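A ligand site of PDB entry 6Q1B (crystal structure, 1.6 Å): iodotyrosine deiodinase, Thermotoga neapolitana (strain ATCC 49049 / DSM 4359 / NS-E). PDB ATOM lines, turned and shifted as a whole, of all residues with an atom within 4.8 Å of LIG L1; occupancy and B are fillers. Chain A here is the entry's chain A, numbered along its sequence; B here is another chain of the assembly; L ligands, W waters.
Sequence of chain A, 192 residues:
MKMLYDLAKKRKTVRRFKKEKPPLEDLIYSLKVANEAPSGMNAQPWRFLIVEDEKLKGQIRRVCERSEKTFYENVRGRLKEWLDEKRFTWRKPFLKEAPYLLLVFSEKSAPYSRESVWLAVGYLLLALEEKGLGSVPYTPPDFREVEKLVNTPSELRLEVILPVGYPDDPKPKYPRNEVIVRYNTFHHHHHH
The side-chain hydroxyl (OG1) of Thr 13 is in hydrogen-bond range of an oxygen (O6) of LIG L1, 3.0 Å away.
O2 of LIG L1 lies within hydrogen-bond range of N of Thr 139, at 3.1 Å.
A nitrogen (N1) of LG2 L2 is in hydrogen-bond range of the backbone carbonyl oxygen of Thr 139, 3.2 Å away.
The guanidinium group (NE) of Arg 15 sits at hydrogen-bond distance from an oxygen (O1) of LIG L1, 2.7 Å away.
O4 of LIG L1 is in hydrogen-bond range of N of Ser 39 of chain B, at 3.2 Å.
An oxygen (O4) of LIG L1 lies close to the backbone carbonyl oxygen of Ser 39 of chain B.
O9 of LIG L1 lies within hydrogen-bond range of N of Tyr 174, 2.8 Å away.
The guanidinium group of Arg 176 is in salt-bridge range of an oxygen (O8) of LIG L1.
N of Thr 13 is in hydrogen-bond range of O7 of LIG L1, at 3.0 Å.
O of Pro 137 lies close to N3 of LIG L1, at 2.7 Å.
The backbone NH (N) of Met 41 of chain B sits at hydrogen-bond distance from an oxygen (O3) of LG2 L2 (2.8 Å).
A nitrogen (N1) of LG2 L2 is in salt-bridge range of the side-chain carboxylate of Glu 68 (2.7 Å).
OG1 of Thr 139 is in hydrogen-bond range of N3 of LIG L1, 3.0 Å away.
An oxygen (O3) of LIG L1 sits at hydrogen-bond distance from an oxygen (O3) of LG2 L2 (2.5 Å).
The side-chain hydroxyl (OH) of Tyr 112 of chain B is in hydrogen-bond range of the backbone carbonyl oxygen (O) of Thr 139.
The side-chain hydroxyl (OG) of Ser 116 of chain B is in hydrogen-bond range of the backbone carbonyl oxygen (O) of Tyr 112 of chain B (2.7 Å).
The guanidinium group (NH1) of Arg 176 sits at hydrogen-bond distance from the side-chain amide oxygen (OD1) of Asn 42 of chain B, at 3.2 Å.
The side-chain amino group of Lys 173 lies within hydrogen-bond range of the backbone carbonyl oxygen of Arg 11.
OG of Ser 116 of chain B is in hydrogen-bond range of N of Gly 40 of chain B.
The backbone carbonyl oxygen of Tyr 174 is in hydrogen-bond range of the guanidinium group of Arg 176, at 3.1 Å.
The backbone carbonyl oxygen (O) of Glu 36 of chain B is in hydrogen-bond range of the guanidinium group (NH2) of Arg 176, at 3.2 Å.
The indole nitrogen (NE1) of Trp 118 lies within hydrogen-bond range of the side-chain carboxylate (OE2) of Glu 115 of chain B.
Lys 12 touches LIG L1 (CB to O7, 3.3 Å).
Trp 82 touches LIG L1 (CH2 to O3, 3.6 Å).
Phe 88 touches LIG L1 (CE2 to O1, 3.3 Å).
Trp 118 touches LIG L1 (CZ3 to C7, 3.8 Å).
CG2 of Val 136 touches N1 of LIG L1, at 3.4 Å.
CD1 of Tyr 138 touches O2 of LIG L1, at 3.5 Å.
Lys 173 touches LIG L1 (CG to O9, 3.3 Å).
Pro 38 of chain B touches LIG L1.
Gly 40 of chain B touches LIG L1.
Asn 42 of chain B touches LIG L1.
Tyr 112 of chain B touches LIG L1.
Glu 115 of chain B touches LIG L1 (OE1 to C7, 3.6 Å).
OG of Ser 116 of chain B touches C9 of LIG L1, at 3.4 Å.
Hydrophobic or aromatic side chains within 4 Å of LIG L1: Trp 82, Phe 88, Trp 118, Val 136, Pro 137, Tyr 138, Tyr 174, Pro 38 of chain B and Tyr 112 of chain B.
Within 4 Å of LIG L1: Lys 12, Thr 13, Arg 15, Trp 82, Phe 88, Trp 118, Val 136, Pro 137, Tyr 138, Thr 139, Lys 173, Tyr 174, Arg 176, Pro 38 of chain B, Ser 39 of chain B, Gly 40 of chain B, Asn 42 of chain B, Tyr 112 of chain B, Glu 115 of chain B and Ser 116 of chain B.
Along chain A the residues within 4 Å of LIG L1 span positions 12 to 176.
The nearest printed residue that does not touch LIG L1 is Leu 119 of chain B (4.1 Å).
Water W1 lies within hydrogen-bond range of O8 of LIG L1 (2.5 Å), NH1 of Arg 11 (2.8 Å), NH2 of Arg 176 (3.4 Å) and O of Glu 36 of chain B (3.5 Å).
Water W4 bridges an oxygen (O7) of LIG L1 (2.6 Å) and the backbone carbonyl oxygen (O) of Pro 172 (2.9 Å).
Water W3 lies within hydrogen-bond range of OG1 of Thr 13 (2.6 Å), O5 of LIG L1 (2.7 Å) and NH1 of Arg 15 (2.9 Å).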
ATOM      1  N   ARG A  11      25.057  29.629  -6.133  1.00  0.00           N
ATOM      2  CA  ARG A  11      25.552  29.101  -7.352  1.00  0.00           C
ATOM      3  C   ARG A  11      24.780  27.859  -7.715  1.00  0.00           C
ATOM      4  O   ARG A  11      24.561  26.978  -6.904  1.00  0.00           O
ATOM      5  CB  ARG A  11      27.019  28.801  -7.245  1.00  0.00           C
ATOM      6  CG  ARG A  11      27.576  28.453  -8.586  1.00  0.00           C
ATOM      7  CD  ARG A  11      27.975  27.036  -8.700  1.00  0.00           C
ATOM      8  NE  ARG A  11      28.146  26.741 -10.102  1.00  0.00           N
ATOM      9  CZ  ARG A  11      27.642  25.699 -10.733  1.00  0.00           C
ATOM     10  NH1 ARG A  11      26.971  24.761 -10.071  1.00  0.00           N
ATOM     11  NH2 ARG A  11      27.858  25.568 -12.019  1.00  0.00           N
ATOM     12  N   LYS A  12      24.365  27.843  -8.976  1.00  0.00           N
ATOM     13  CA  LYS A  12      23.607  26.769  -9.536  1.00  0.00           C
ATOM     14  C   LYS A  12      23.995  26.585 -10.973  1.00  0.00           C
ATOM     15  O   LYS A  12      24.686  27.396 -11.574  1.00  0.00           O
ATOM     16  CB  LYS A  12      22.134  27.064  -9.458  1.00  0.00           C
ATOM     17  CG  LYS A  12      21.708  28.275 -10.238  1.00  0.00           C
ATOM     18  CD  LYS A  12      20.217  28.461 -10.110  1.00  0.00           C
ATOM     19  CE  LYS A  12      19.684  29.614 -10.951  1.00  0.00           C
ATOM     20  NZ  LYS A  12      20.079  30.942 -10.426  1.00  0.00           N
ATOM     21  N   THR A  13      23.515  25.493 -11.518  1.00  0.00           N
ATOM     22  CA  THR A  13      23.796  25.190 -12.890  1.00  0.00           C
ATOM     23  C   THR A  13      23.240  26.252 -13.773  1.00  0.00           C
ATOM     24  O   THR A  13      22.118  26.728 -13.582  1.00  0.00           O
ATOM     25  CB  THR A  13      23.170  23.864 -13.340  1.00  0.00           C
ATOM     26  OG1 THR A  13      23.274  22.900 -12.293  1.00  0.00           O
ATOM     27  CG2 THR A  13      23.861  23.352 -14.541  1.00  0.00           C
ATOM     28  N   ARG A  15      22.570  26.376 -17.756  1.00  0.00           N
ATOM     29  CA  ARG A  15      22.558  25.725 -19.042  1.00  0.00           C
ATOM     30  C   ARG A  15      21.991  26.620 -20.107  1.00  0.00           C
ATOM     31  O   ARG A  15      21.896  26.220 -21.283  1.00  0.00           O
ATOM     32  CB  ARG A  15      21.754  24.443 -18.993  1.00  0.00           C
ATOM     33  CG  ARG A  15      22.354  23.442 -18.052  1.00  0.00           C
ATOM     34  CD  ARG A  15      21.616  22.146 -18.086  1.00  0.00           C
ATOM     35  NE  ARG A  15      22.176  21.166 -17.169  1.00  0.00           N
ATOM     36  CZ  ARG A  15      21.805  21.010 -15.897  1.00  0.00           C
ATOM     37  NH1 ARG A  15      20.878  21.787 -15.354  1.00  0.00           N
ATOM     38  NH2 ARG A  15      22.379  20.092 -15.152  1.00  0.00           N
ATOM     39  N   GLU A  68      25.858  11.640 -26.277  1.00  0.00           N
ATOM     40  CA  GLU A  68      24.708  11.721 -25.395  1.00  0.00           C
ATOM     41  C   GLU A  68      23.540  10.951 -25.939  1.00  0.00           C
ATOM     42  O   GLU A  68      22.873  10.224 -25.225  1.00  0.00           O
ATOM     43  CB  GLU A  68      24.256  13.160 -25.169  1.00  0.00           C
ATOM     44  CG  GLU A  68      25.253  13.981 -24.393  1.00  0.00           C
ATOM     45  CD  GLU A  68      25.447  13.523 -22.973  1.00  0.00           C
ATOM     46  OE1 GLU A  68      24.903  12.462 -22.561  1.00  0.00           O
ATOM     47  OE2 GLU A  68      26.171  14.247 -22.252  1.00  0.00           O
ATOM     48  N   TRP A  82      16.495  10.049 -13.059  1.00  0.00           N
ATOM     49  CA  TRP A  82      16.708  11.424 -12.724  1.00  0.00           C
ATOM     50  C   TRP A  82      16.660  12.279 -13.973  1.00  0.00           C
ATOM     51  O   TRP A  82      16.038  13.331 -13.992  1.00  0.00           O
ATOM     52  CB  TRP A  82      18.061  11.559 -12.038  1.00  0.00           C
ATOM     53  CG  TRP A  82      18.362  12.922 -11.523  1.00  0.00           C
ATOM     54  CD1 TRP A  82      17.995  13.431 -10.326  1.00  0.00           C
ATOM     55  CD2 TRP A  82      19.095  13.936 -12.191  1.00  0.00           C
ATOM     56  NE1 TRP A  82      18.447  14.709 -10.196  1.00  0.00           N
ATOM     57  CE2 TRP A  82      19.144  15.045 -11.322  1.00  0.00           C
ATOM     58  CE3 TRP A  82      19.718  14.025 -13.433  1.00  0.00           C
ATOM     59  CZ2 TRP A  82      19.783  16.218 -11.656  1.00  0.00           C
ATOM     60  CZ3 TRP A  82      20.379  15.195 -13.765  1.00  0.00           C
ATOM     61  CH2 TRP A  82      20.394  16.282 -12.872  1.00  0.00           C
ATOM     62  N   PHE A  88      15.778  15.972 -19.160  1.00  0.00           N
ATOM     63  CA  PHE A  88      17.019  16.087 -19.898  1.00  0.00           C
ATOM     64  C   PHE A  88      16.942  15.353 -21.208  1.00  0.00           C
ATOM     65  O   PHE A  88      16.234  14.340 -21.331  1.00  0.00           O
ATOM     66  CB  PHE A  88      18.179  15.503 -19.099  1.00  0.00           C
ATOM     67  CG  PHE A  88      18.709  16.408 -18.048  1.00  0.00           C
ATOM     68  CD1 PHE A  88      17.981  16.703 -16.932  1.00  0.00           C
ATOM     69  CD2 PHE A  88      19.959  16.950 -18.165  1.00  0.00           C
ATOM     70  CE1 PHE A  88      18.481  17.533 -15.954  1.00  0.00           C
ATOM     71  CE2 PHE A  88      20.461  17.762 -17.199  1.00  0.00           C
ATOM     72  CZ  PHE A  88      19.728  18.064 -16.111  1.00  0.00           C
ATOM     73  N   PHE A  94      23.688  24.409 -25.207  1.00  0.00           N
ATOM     74  CA  PHE A  94      24.506  25.333 -24.481  1.00  0.00           C
ATOM     75  C   PHE A  94      25.936  25.185 -24.930  1.00  0.00           C
ATOM     76  O   PHE A  94      26.725  26.071 -24.676  1.00  0.00           O
ATOM     77  CB  PHE A  94      24.425  25.134 -22.972  1.00  0.00           C
ATOM     78  CG  PHE A  94      24.655  23.725 -22.509  1.00  0.00           C
ATOM     79  CD1 PHE A  94      25.920  23.205 -22.397  1.00  0.00           C
ATOM     80  CD2 PHE A  94      23.568  22.920 -22.149  1.00  0.00           C
ATOM     81  CE1 PHE A  94      26.125  21.913 -21.966  1.00  0.00           C
ATOM     82  CE2 PHE A  94      23.754  21.624 -21.716  1.00  0.00           C
ATOM     83  CZ  PHE A  94      25.025  21.114 -21.610  1.00  0.00           C
ATOM     84  N   TRP A 118      39.482  18.409 -10.030  1.00  0.00           N
ATOM     85  CA  TRP A 118      38.075  18.589  -9.667  1.00  0.00           C
ATOM     86  C   TRP A 118      37.938  19.489  -8.466  1.00  0.00           C
ATOM     87  O   TRP A 118      37.019  20.289  -8.395  1.00  0.00           O
ATOM     88  CB  TRP A 118      37.401  17.245  -9.466  1.00  0.00           C
ATOM     89  CG  TRP A 118      37.034  16.776 -10.793  1.00  0.00           C
ATOM     90  CD1 TRP A 118      37.727  15.937 -11.581  1.00  0.00           C
ATOM     91  CD2 TRP A 118      35.913  17.228 -11.552  1.00  0.00           C
ATOM     92  NE1 TRP A 118      37.089  15.802 -12.792  1.00  0.00           N
ATOM     93  CE2 TRP A 118      35.976  16.589 -12.798  1.00  0.00           C
ATOM     94  CE3 TRP A 118      34.860  18.109 -11.300  1.00  0.00           C
ATOM     95  CZ2 TRP A 118      34.983  16.767 -13.778  1.00  0.00           C
ATOM     96  CZ3 TRP A 118      33.896  18.299 -12.276  1.00  0.00           C
ATOM     97  CH2 TRP A 118      33.979  17.630 -13.504  1.00  0.00           C
ATOM     98  N   VAL A 136      28.208  24.914 -16.221  1.00  0.00           N
ATOM     99  CA  VAL A 136      27.708  23.597 -15.905  1.00  0.00           C
ATOM    100  C   VAL A 136      28.886  22.680 -16.146  1.00  0.00           C
ATOM    101  O   VAL A 136      29.577  22.824 -17.141  1.00  0.00           O
ATOM    102  CB  VAL A 136      26.503  23.218 -16.750  1.00  0.00           C
ATOM    103  CG1 VAL A 136      26.751  23.478 -18.209  1.00  0.00           C
ATOM    104  CG2 VAL A 136      26.124  21.770 -16.484  1.00  0.00           C
ATOM    105  N   PRO A 137      29.156  21.780 -15.211  1.00  0.00           N
ATOM    106  CA  PRO A 137      30.210  20.826 -15.445  1.00  0.00           C
ATOM    107  C   PRO A 137      29.670  19.800 -16.406  1.00  0.00           C
ATOM    108  O   PRO A 137      28.966  18.899 -16.018  1.00  0.00           O
ATOM    109  CB  PRO A 137      30.495  20.242 -14.068  1.00  0.00           C
ATOM    110  CG  PRO A 137      29.920  21.220 -13.126  1.00  0.00           C
ATOM    111  CD  PRO A 137      28.726  21.753 -13.806  1.00  0.00           C
ATOM    112  N   TYR A 138      29.954  19.984 -17.661  1.00  0.00           N
ATOM    113  CA  TYR A 138      29.349  19.121 -18.635  1.00  0.00           C
ATOM    114  C   TYR A 138      30.298  17.984 -18.918  1.00  0.00           C
ATOM    115  O   TYR A 138      31.449  18.200 -19.255  1.00  0.00           O
ATOM    116  CB  TYR A 138      28.994  19.867 -19.898  1.00  0.00           C
ATOM    117  CG  TYR A 138      28.537  18.893 -20.921  1.00  0.00           C
ATOM    118  CD1 TYR A 138      27.399  18.130 -20.712  1.00  0.00           C
ATOM    119  CD2 TYR A 138      29.277  18.661 -22.060  1.00  0.00           C
ATOM    120  CE1 TYR A 138      27.012  17.189 -21.614  1.00  0.00           C
ATOM    121  CE2 TYR A 138      28.909  17.725 -22.964  1.00  0.00           C
ATOM    122  CZ  TYR A 138      27.762  16.996 -22.752  1.00  0.00           C
ATOM    123  OH  TYR A 138      27.384  16.058 -23.655  1.00  0.00           O
ATOM    124  N   THR A 139      29.786  16.768 -18.819  1.00  0.00           N
ATOM    125  CA  THR A 139      30.590  15.583 -18.952  1.00  0.00           C
ATOM    126  C   THR A 139      29.876  14.659 -19.928  1.00  0.00           C
ATOM    127  O   THR A 139      28.970  13.931 -19.539  1.00  0.00           O
ATOM    128  CB  THR A 139      30.785  14.886 -17.617  1.00  0.00           C
ATOM    129  OG1 THR A 139      29.514  14.657 -17.021  1.00  0.00           O
ATOM    130  CG2 THR A 139      31.615  15.748 -16.672  1.00  0.00           C
ATOM    131  N   PRO A 140      30.239  14.724 -21.207  1.00  0.00           N
ATOM    132  CA  PRO A 140      29.646  13.814 -22.188  1.00  0.00           C
ATOM    133  C   PRO A 140      30.087  12.400 -21.879  1.00  0.00           C
ATOM    134  O   PRO A 140      31.087  12.219 -21.183  1.00  0.00           O
ATOM    135  CB  PRO A 140      30.218  14.299 -23.503  1.00  0.00           C
ATOM    136  CG  PRO A 140      31.533  14.904 -23.127  1.00  0.00           C
ATOM    137  CD  PRO A 140      31.319  15.533 -21.787  1.00  0.00           C
ATOM    138  N   PRO A 172      15.950  27.070 -11.655  1.00  0.00           N
ATOM    139  CA  PRO A 172      16.330  27.128 -10.258  1.00  0.00           C
ATOM    140  C   PRO A 172      17.213  25.985  -9.839  1.00  0.00           C
ATOM    141  O   PRO A 172      17.226  24.897 -10.432  1.00  0.00           O
ATOM    142  CB  PRO A 172      14.995  27.048  -9.530  1.00  0.00           C
ATOM    143  CG  PRO A 172      14.014  27.529 -10.532  1.00  0.00           C
ATOM    144  CD  PRO A 172      14.492  27.101 -11.841  1.00  0.00           C
ATOM    145  N   LYS A 173      17.976  26.280  -8.796  1.00  0.00           N
ATOM    146  CA  LYS A 173      18.854  25.328  -8.186  1.00  0.00           C
ATOM    147  C   LYS A 173      18.042  24.160  -7.720  1.00  0.00           C
ATOM    148  O   LYS A 173      16.906  24.356  -7.234  1.00  0.00           O
ATOM    149  CB  LYS A 173      19.561  25.964  -7.037  1.00  0.00           C
ATOM    150  CG  LYS A 173      20.701  25.146  -6.554  1.00  0.00           C
ATOM    151  CD  LYS A 173      21.591  25.920  -5.651  1.00  0.00           C
ATOM    152  CE  LYS A 173      22.740  25.039  -5.305  1.00  0.00           C
ATOM    153  NZ  LYS A 173      23.809  25.694  -4.548  1.00  0.00           N
ATOM    154  N   TYR A 174      18.558  22.954  -7.869  1.00  0.00           N
ATOM    155  CA  TYR A 174      17.867  21.798  -7.327  1.00  0.00           C
ATOM    156  C   TYR A 174      18.073  21.772  -5.829  1.00  0.00           C
ATOM    157  O   TYR A 174      18.910  22.464  -5.270  1.00  0.00           O
ATOM    158  CB  TYR A 174      18.392  20.526  -7.956  1.00  0.00           C
ATOM    159  CG  TYR A 174      18.214  20.449  -9.442  1.00  0.00           C
ATOM    160  CD1 TYR A 174      17.198  21.160 -10.080  1.00  0.00           C
ATOM    161  CD2 TYR A 174      19.035  19.649 -10.214  1.00  0.00           C
ATOM    162  CE1 TYR A 174      17.031  21.073 -11.422  1.00  0.00           C
ATOM    163  CE2 TYR A 174      18.877  19.564 -11.557  1.00  0.00           C
ATOM    164  CZ  TYR A 174      17.875  20.276 -12.161  1.00  0.00           C
ATOM    165  OH  TYR A 174      17.733  20.172 -13.505  1.00  0.00           O
ATOM    166  N   ARG A 176      18.984  20.576  -1.996  1.00  0.00           N
ATOM    167  CA  ARG A 176      20.051  19.869  -1.359  1.00  0.00           C
ATOM    168  C   ARG A 176      19.529  19.190  -0.141  1.00  0.00           C
ATOM    169  O   ARG A 176      18.894  19.801   0.719  1.00  0.00           O
ATOM    170  CB  ARG A 176      21.185  20.815  -0.972  1.00  0.00           C
ATOM    171  CG  ARG A 176      21.869  21.470  -2.116  1.00  0.00           C
ATOM    172  CD  ARG A 176      22.631  20.446  -2.913  1.00  0.00           C
ATOM    173  NE  ARG A 176      23.510  21.020  -3.916  1.00  0.00           N
ATOM    174  CZ  ARG A 176      23.107  21.482  -5.079  1.00  0.00           C
ATOM    175  NH1 ARG A 176      21.811  21.510  -5.386  1.00  0.00           N
ATOM    176  NH2 ARG A 176      24.001  21.944  -5.950  1.00  0.00           N
ATOM    177  N   GLU B  36      26.521  22.518  -0.875  1.00  0.00           N
ATOM    178  CA  GLU B  36      25.865  23.340  -1.889  1.00  0.00           C
ATOM    179  C   GLU B  36      26.475  23.181  -3.243  1.00  0.00           C
ATOM    180  O   GLU B  36      25.970  23.720  -4.233  1.00  0.00           O
ATOM    181  CB  GLU B  36      25.924  24.809  -1.508  1.00  0.00           C
ATOM    182  CG  GLU B  36      25.089  25.106  -0.327  1.00  0.00           C
ATOM    183  CD  GLU B  36      23.638  24.904  -0.611  1.00  0.00           C
ATOM    184  OE1 GLU B  36      23.225  25.128  -1.766  1.00  0.00           O
ATOM    185  OE2 GLU B  36      22.892  24.502   0.321  1.00  0.00           O
ATOM    186  N   PRO B  38      27.678  21.562  -6.737  1.00  0.00           N
ATOM    187  CA  PRO B  38      27.036  20.717  -7.721  1.00  0.00           C
ATOM    188  C   PRO B  38      27.551  19.321  -7.615  1.00  0.00           C
ATOM    189  O   PRO B  38      28.576  19.051  -6.983  1.00  0.00           O
ATOM    190  CB  PRO B  38      27.459  21.330  -9.042  1.00  0.00           C
ATOM    191  CG  PRO B  38      28.769  21.953  -8.756  1.00  0.00           C
ATOM    192  CD  PRO B  38      28.626  22.487  -7.373  1.00  0.00           C
ATOM    193  N   SER B  39      26.818  18.409  -8.220  1.00  0.00           N
ATOM    194  CA  SER B  39      27.248  17.053  -8.287  1.00  0.00           C
ATOM    195  C   SER B  39      26.520  16.389  -9.409  1.00  0.00           C
ATOM    196  O   SER B  39      25.461  16.851  -9.828  1.00  0.00           O
ATOM    197  CB  SER B  39      27.002  16.312  -6.982  1.00  0.00           C
ATOM    198  OG  SER B  39      25.630  16.305  -6.651  1.00  0.00           O
ATOM    199  N   GLY B  40      27.096  15.307  -9.902  1.00  0.00           N
ATOM    200  CA  GLY B  40      26.455  14.548 -10.947  1.00  0.00           C
ATOM    201  C   GLY B  40      25.078  14.110 -10.466  1.00  0.00           C
ATOM    202  O   GLY B  40      24.925  13.594  -9.366  1.00  0.00           O
ATOM    203  N   MET B  41      24.101  14.324 -11.329  1.00  0.00           N
ATOM    204  CA  MET B  41      22.669  14.109 -11.078  1.00  0.00           C
ATOM    205  C   MET B  41      22.215  14.592  -9.707  1.00  0.00           C
ATOM    206  O   MET B  41      21.227  14.103  -9.144  1.00  0.00           O
ATOM    207  CB  MET B  41      22.297  12.640 -11.294  1.00  0.00           C
ATOM    208  CG  MET B  41      22.801  11.623 -10.323  1.00  0.00           C
ATOM    209  SD  MET B  41      21.837  10.108 -10.548  1.00  0.00           S
ATOM    210  CE  MET B  41      20.385  10.506  -9.586  1.00  0.00           C
ATOM    211  N   ASN B  42      22.881  15.657  -9.235  1.00  0.00           N
ATOM    212  CA  ASN B  42      22.626  16.260  -7.939  1.00  0.00           C
ATOM    213  C   ASN B  42      22.548  15.213  -6.849  1.00  0.00           C
ATOM    214  O   ASN B  42      21.795  15.334  -5.877  1.00  0.00           O
ATOM    215  CB  ASN B  42      21.346  17.081  -7.956  1.00  0.00           C
ATOM    216  CG  ASN B  42      21.208  17.953  -6.740  1.00  0.00           C
ATOM    217  OD1 ASN B  42      22.181  18.462  -6.225  1.00  0.00           O
ATOM    218  ND2 ASN B  42      19.985  18.084  -6.254  1.00  0.00           N
ATOM    219  N   TYR B 112      29.563  10.227 -11.462  1.00  0.00           N
ATOM    220  CA  TYR B 112      30.611  11.202 -11.287  1.00  0.00           C
ATOM    221  C   TYR B 112      30.770  11.543  -9.812  1.00  0.00           C
ATOM    222  O   TYR B 112      31.011  12.704  -9.449  1.00  0.00           O
ATOM    223  CB  TYR B 112      30.307  12.454 -12.088  1.00  0.00           C
ATOM    224  CG  TYR B 112      29.907  12.177 -13.523  1.00  0.00           C
ATOM    225  CD1 TYR B 112      30.848  11.792 -14.457  1.00  0.00           C
ATOM    226  CD2 TYR B 112      28.589  12.315 -13.938  1.00  0.00           C
ATOM    227  CE1 TYR B 112      30.486  11.547 -15.772  1.00  0.00           C
ATOM    228  CE2 TYR B 112      28.221  12.060 -15.247  1.00  0.00           C
ATOM    229  CZ  TYR B 112      29.174  11.679 -16.161  1.00  0.00           C
ATOM    230  OH  TYR B 112      28.812  11.434 -17.476  1.00  0.00           O
ATOM    231  N   GLU B 115      34.395  12.979  -8.970  1.00  0.00           N
ATOM    232  CA  GLU B 115      34.520  14.323  -9.481  1.00  0.00           C
ATOM    233  C   GLU B 115      33.740  15.253  -8.609  1.00  0.00           C
ATOM    234  O   GLU B 115      34.193  16.295  -8.221  1.00  0.00           O
ATOM    235  CB  GLU B 115      34.014  14.369 -10.917  1.00  0.00           C
ATOM    236  CG  GLU B 115      34.903  13.543 -11.776  1.00  0.00           C
ATOM    237  CD  GLU B 115      34.469  13.515 -13.215  1.00  0.00           C
ATOM    238  OE1 GLU B 115      33.264  13.694 -13.478  1.00  0.00           O
ATOM    239  OE2 GLU B 115      35.337  13.321 -14.086  1.00  0.00           O
ATOM    240  N   SER B 116      32.522  14.847  -8.292  1.00  0.00           N
ATOM    241  CA  SER B 116      31.664  15.679  -7.504  1.00  0.00           C
ATOM    242  C   SER B 116      32.158  15.898  -6.102  1.00  0.00           C
ATOM    243  O   SER B 116      32.075  16.987  -5.568  1.00  0.00           O
ATOM    244  CB  SER B 116      30.287  15.051  -7.421  1.00  0.00           C
ATOM    245  OG  SER B 116      29.685  14.979  -8.712  1.00  0.00           O
ATOM    246  N   LEU B 119      35.187  18.192  -6.225  1.00  0.00           N
ATOM    247  CA  LEU B 119      34.687  19.523  -6.432  1.00  0.00           C
ATOM    248  C   LEU B 119      34.199  20.107  -5.118  1.00  0.00           C
ATOM    249  O   LEU B 119      34.533  21.196  -4.747  1.00  0.00           O
ATOM    250  CB  LEU B 119      33.582  19.466  -7.466  1.00  0.00           C
ATOM    251  CG  LEU B 119      33.104  20.776  -8.040  1.00  0.00           C
ATOM    252  CD1 LEU B 119      32.459  20.493  -9.362  1.00  0.00           C
ATOM    253  CD2 LEU B 119      32.127  21.489  -7.118  1.00  0.00           C
HETATM  254  N1  LIG L   1      24.856  18.682 -15.948  1.00  0.00           N
HETATM  255  C1  LIG L   1      24.499  18.366 -17.201  1.00  0.00           C
HETATM  256  O1  LIG L   1      23.528  18.927 -17.708  1.00  0.00           O
HETATM  257  N2  LIG L   1      25.197  17.429 -17.911  1.00  0.00           N
HETATM  258  C2  LIG L   1      26.293  16.800 -17.385  1.00  0.00           C
HETATM  259  O2  LIG L   1      26.899  15.961 -18.037  1.00  0.00           O
HETATM  260  C3  LIG L   1      26.654  17.113 -16.097  1.00  0.00           C
HETATM  261  N3  LIG L   1      27.736  16.509 -15.541  1.00  0.00           N
HETATM  262  C4  LIG L   1      28.122  16.870 -14.290  1.00  0.00           C
HETATM  263  C5  LIG L   1      29.254  16.259 -13.774  1.00  0.00           C
HETATM  264  C6  LIG L   1      29.680  16.593 -12.508  1.00  0.00           C
HETATM  265  C7  LIG L   1      30.900  15.933 -11.963  1.00  0.00           C
HETATM  266  C8  LIG L   1      28.963  17.530 -11.787  1.00  0.00           C
HETATM  267  C9  LIG L   1      29.479  17.919 -10.435  1.00  0.00           C
HETATM  268  C10 LIG L   1      27.835  18.165 -12.304  1.00  0.00           C
HETATM  269  C11 LIG L   1      27.412  17.817 -13.575  1.00  0.00           C
HETATM  270  N4  LIG L   1      26.282  18.404 -14.134  1.00  0.00           N
HETATM  271  C12 LIG L   1      25.939  18.068 -15.409  1.00  0.00           C
HETATM  272  C13 LIG L   1      25.482  19.420 -13.414  1.00  0.00           C
HETATM  273  C14 LIG L   1      24.598  18.716 -12.384  1.00  0.00           C
HETATM  274  O3  LIG L   1      23.461  18.178 -13.023  1.00  0.00           O
HETATM  275  C15 LIG L   1      24.231  19.727 -11.295  1.00  0.00           C
HETATM  276  O4  LIG L   1      25.397  20.104 -10.599  1.00  0.00           O
HETATM  277  C16 LIG L   1      23.180  19.199 -10.322  1.00  0.00           C
HETATM  278  O5  LIG L   1      21.993  19.041 -11.061  1.00  0.00           O
HETATM  279  C17 LIG L   1      22.932  20.200  -9.214  1.00  0.00           C
HETATM  280  O6  LIG L   1      22.598  21.424  -9.816  1.00  0.00           O
HETATM  281  P1  LIG L   1      22.256  22.684  -8.913  1.00  0.00           P
HETATM  282  O7  LIG L   1      21.726  23.778  -9.859  1.00  0.00           O
HETATM  283  O8  LIG L   1      23.528  23.146  -8.194  1.00  0.00           O
HETATM  284  O9  LIG L   1      21.199  22.188  -7.923  1.00  0.00           O
HETATM  285  N1  LG2 L   2      25.802  14.059 -19.540  1.00  0.00           N
HETATM  286  C1  LG2 L   2      24.416  13.756 -19.765  1.00  0.00           C
HETATM  287  C2  LG2 L   2      23.732  15.068 -20.069  1.00  0.00           C
HETATM  288  O1  LG2 L   2      22.422  14.979 -20.321  1.00  0.00           O
HETATM  289  O2  LG2 L   2      24.269  16.171 -20.045  1.00  0.00           O
HETATM  290  C3  LG2 L   2      23.747  13.163 -18.541  1.00  0.00           C
HETATM  291  C4  LG2 L   2      23.920  13.907 -17.269  1.00  0.00           C
HETATM  292  C5  LG2 L   2      24.775  13.382 -16.291  1.00  0.00           C
HETATM  293  C6  LG2 L   2      23.200  15.077 -17.000  1.00  0.00           C
HETATM  294  C7  LG2 L   2      24.891  14.045 -15.066  1.00  0.00           C
HETATM  295  C8  LG2 L   2      23.313  15.748 -15.780  1.00  0.00           C
HETATM  296  C9  LG2 L   2      24.184  15.232 -14.818  1.00  0.00           C
HETATM  297  O3  LG2 L   2      24.301  15.870 -13.637  1.00  0.00           O
HETATM  298  F1  LG2 L   2      25.716  13.586 -14.104  1.00  0.00           F
HETATM  299  O   HOH W   1      25.679  24.331  -7.667  1.00  0.00           O
HETATM  300  O   HOH W   2      22.294  19.104 -20.024  1.00  0.00           O
HETATM  301  O   HOH W   3      21.313  21.244 -12.540  1.00  0.00           O
HETATM  302  O   HOH W   4      19.614  23.526 -11.276  1.00  0.00           O
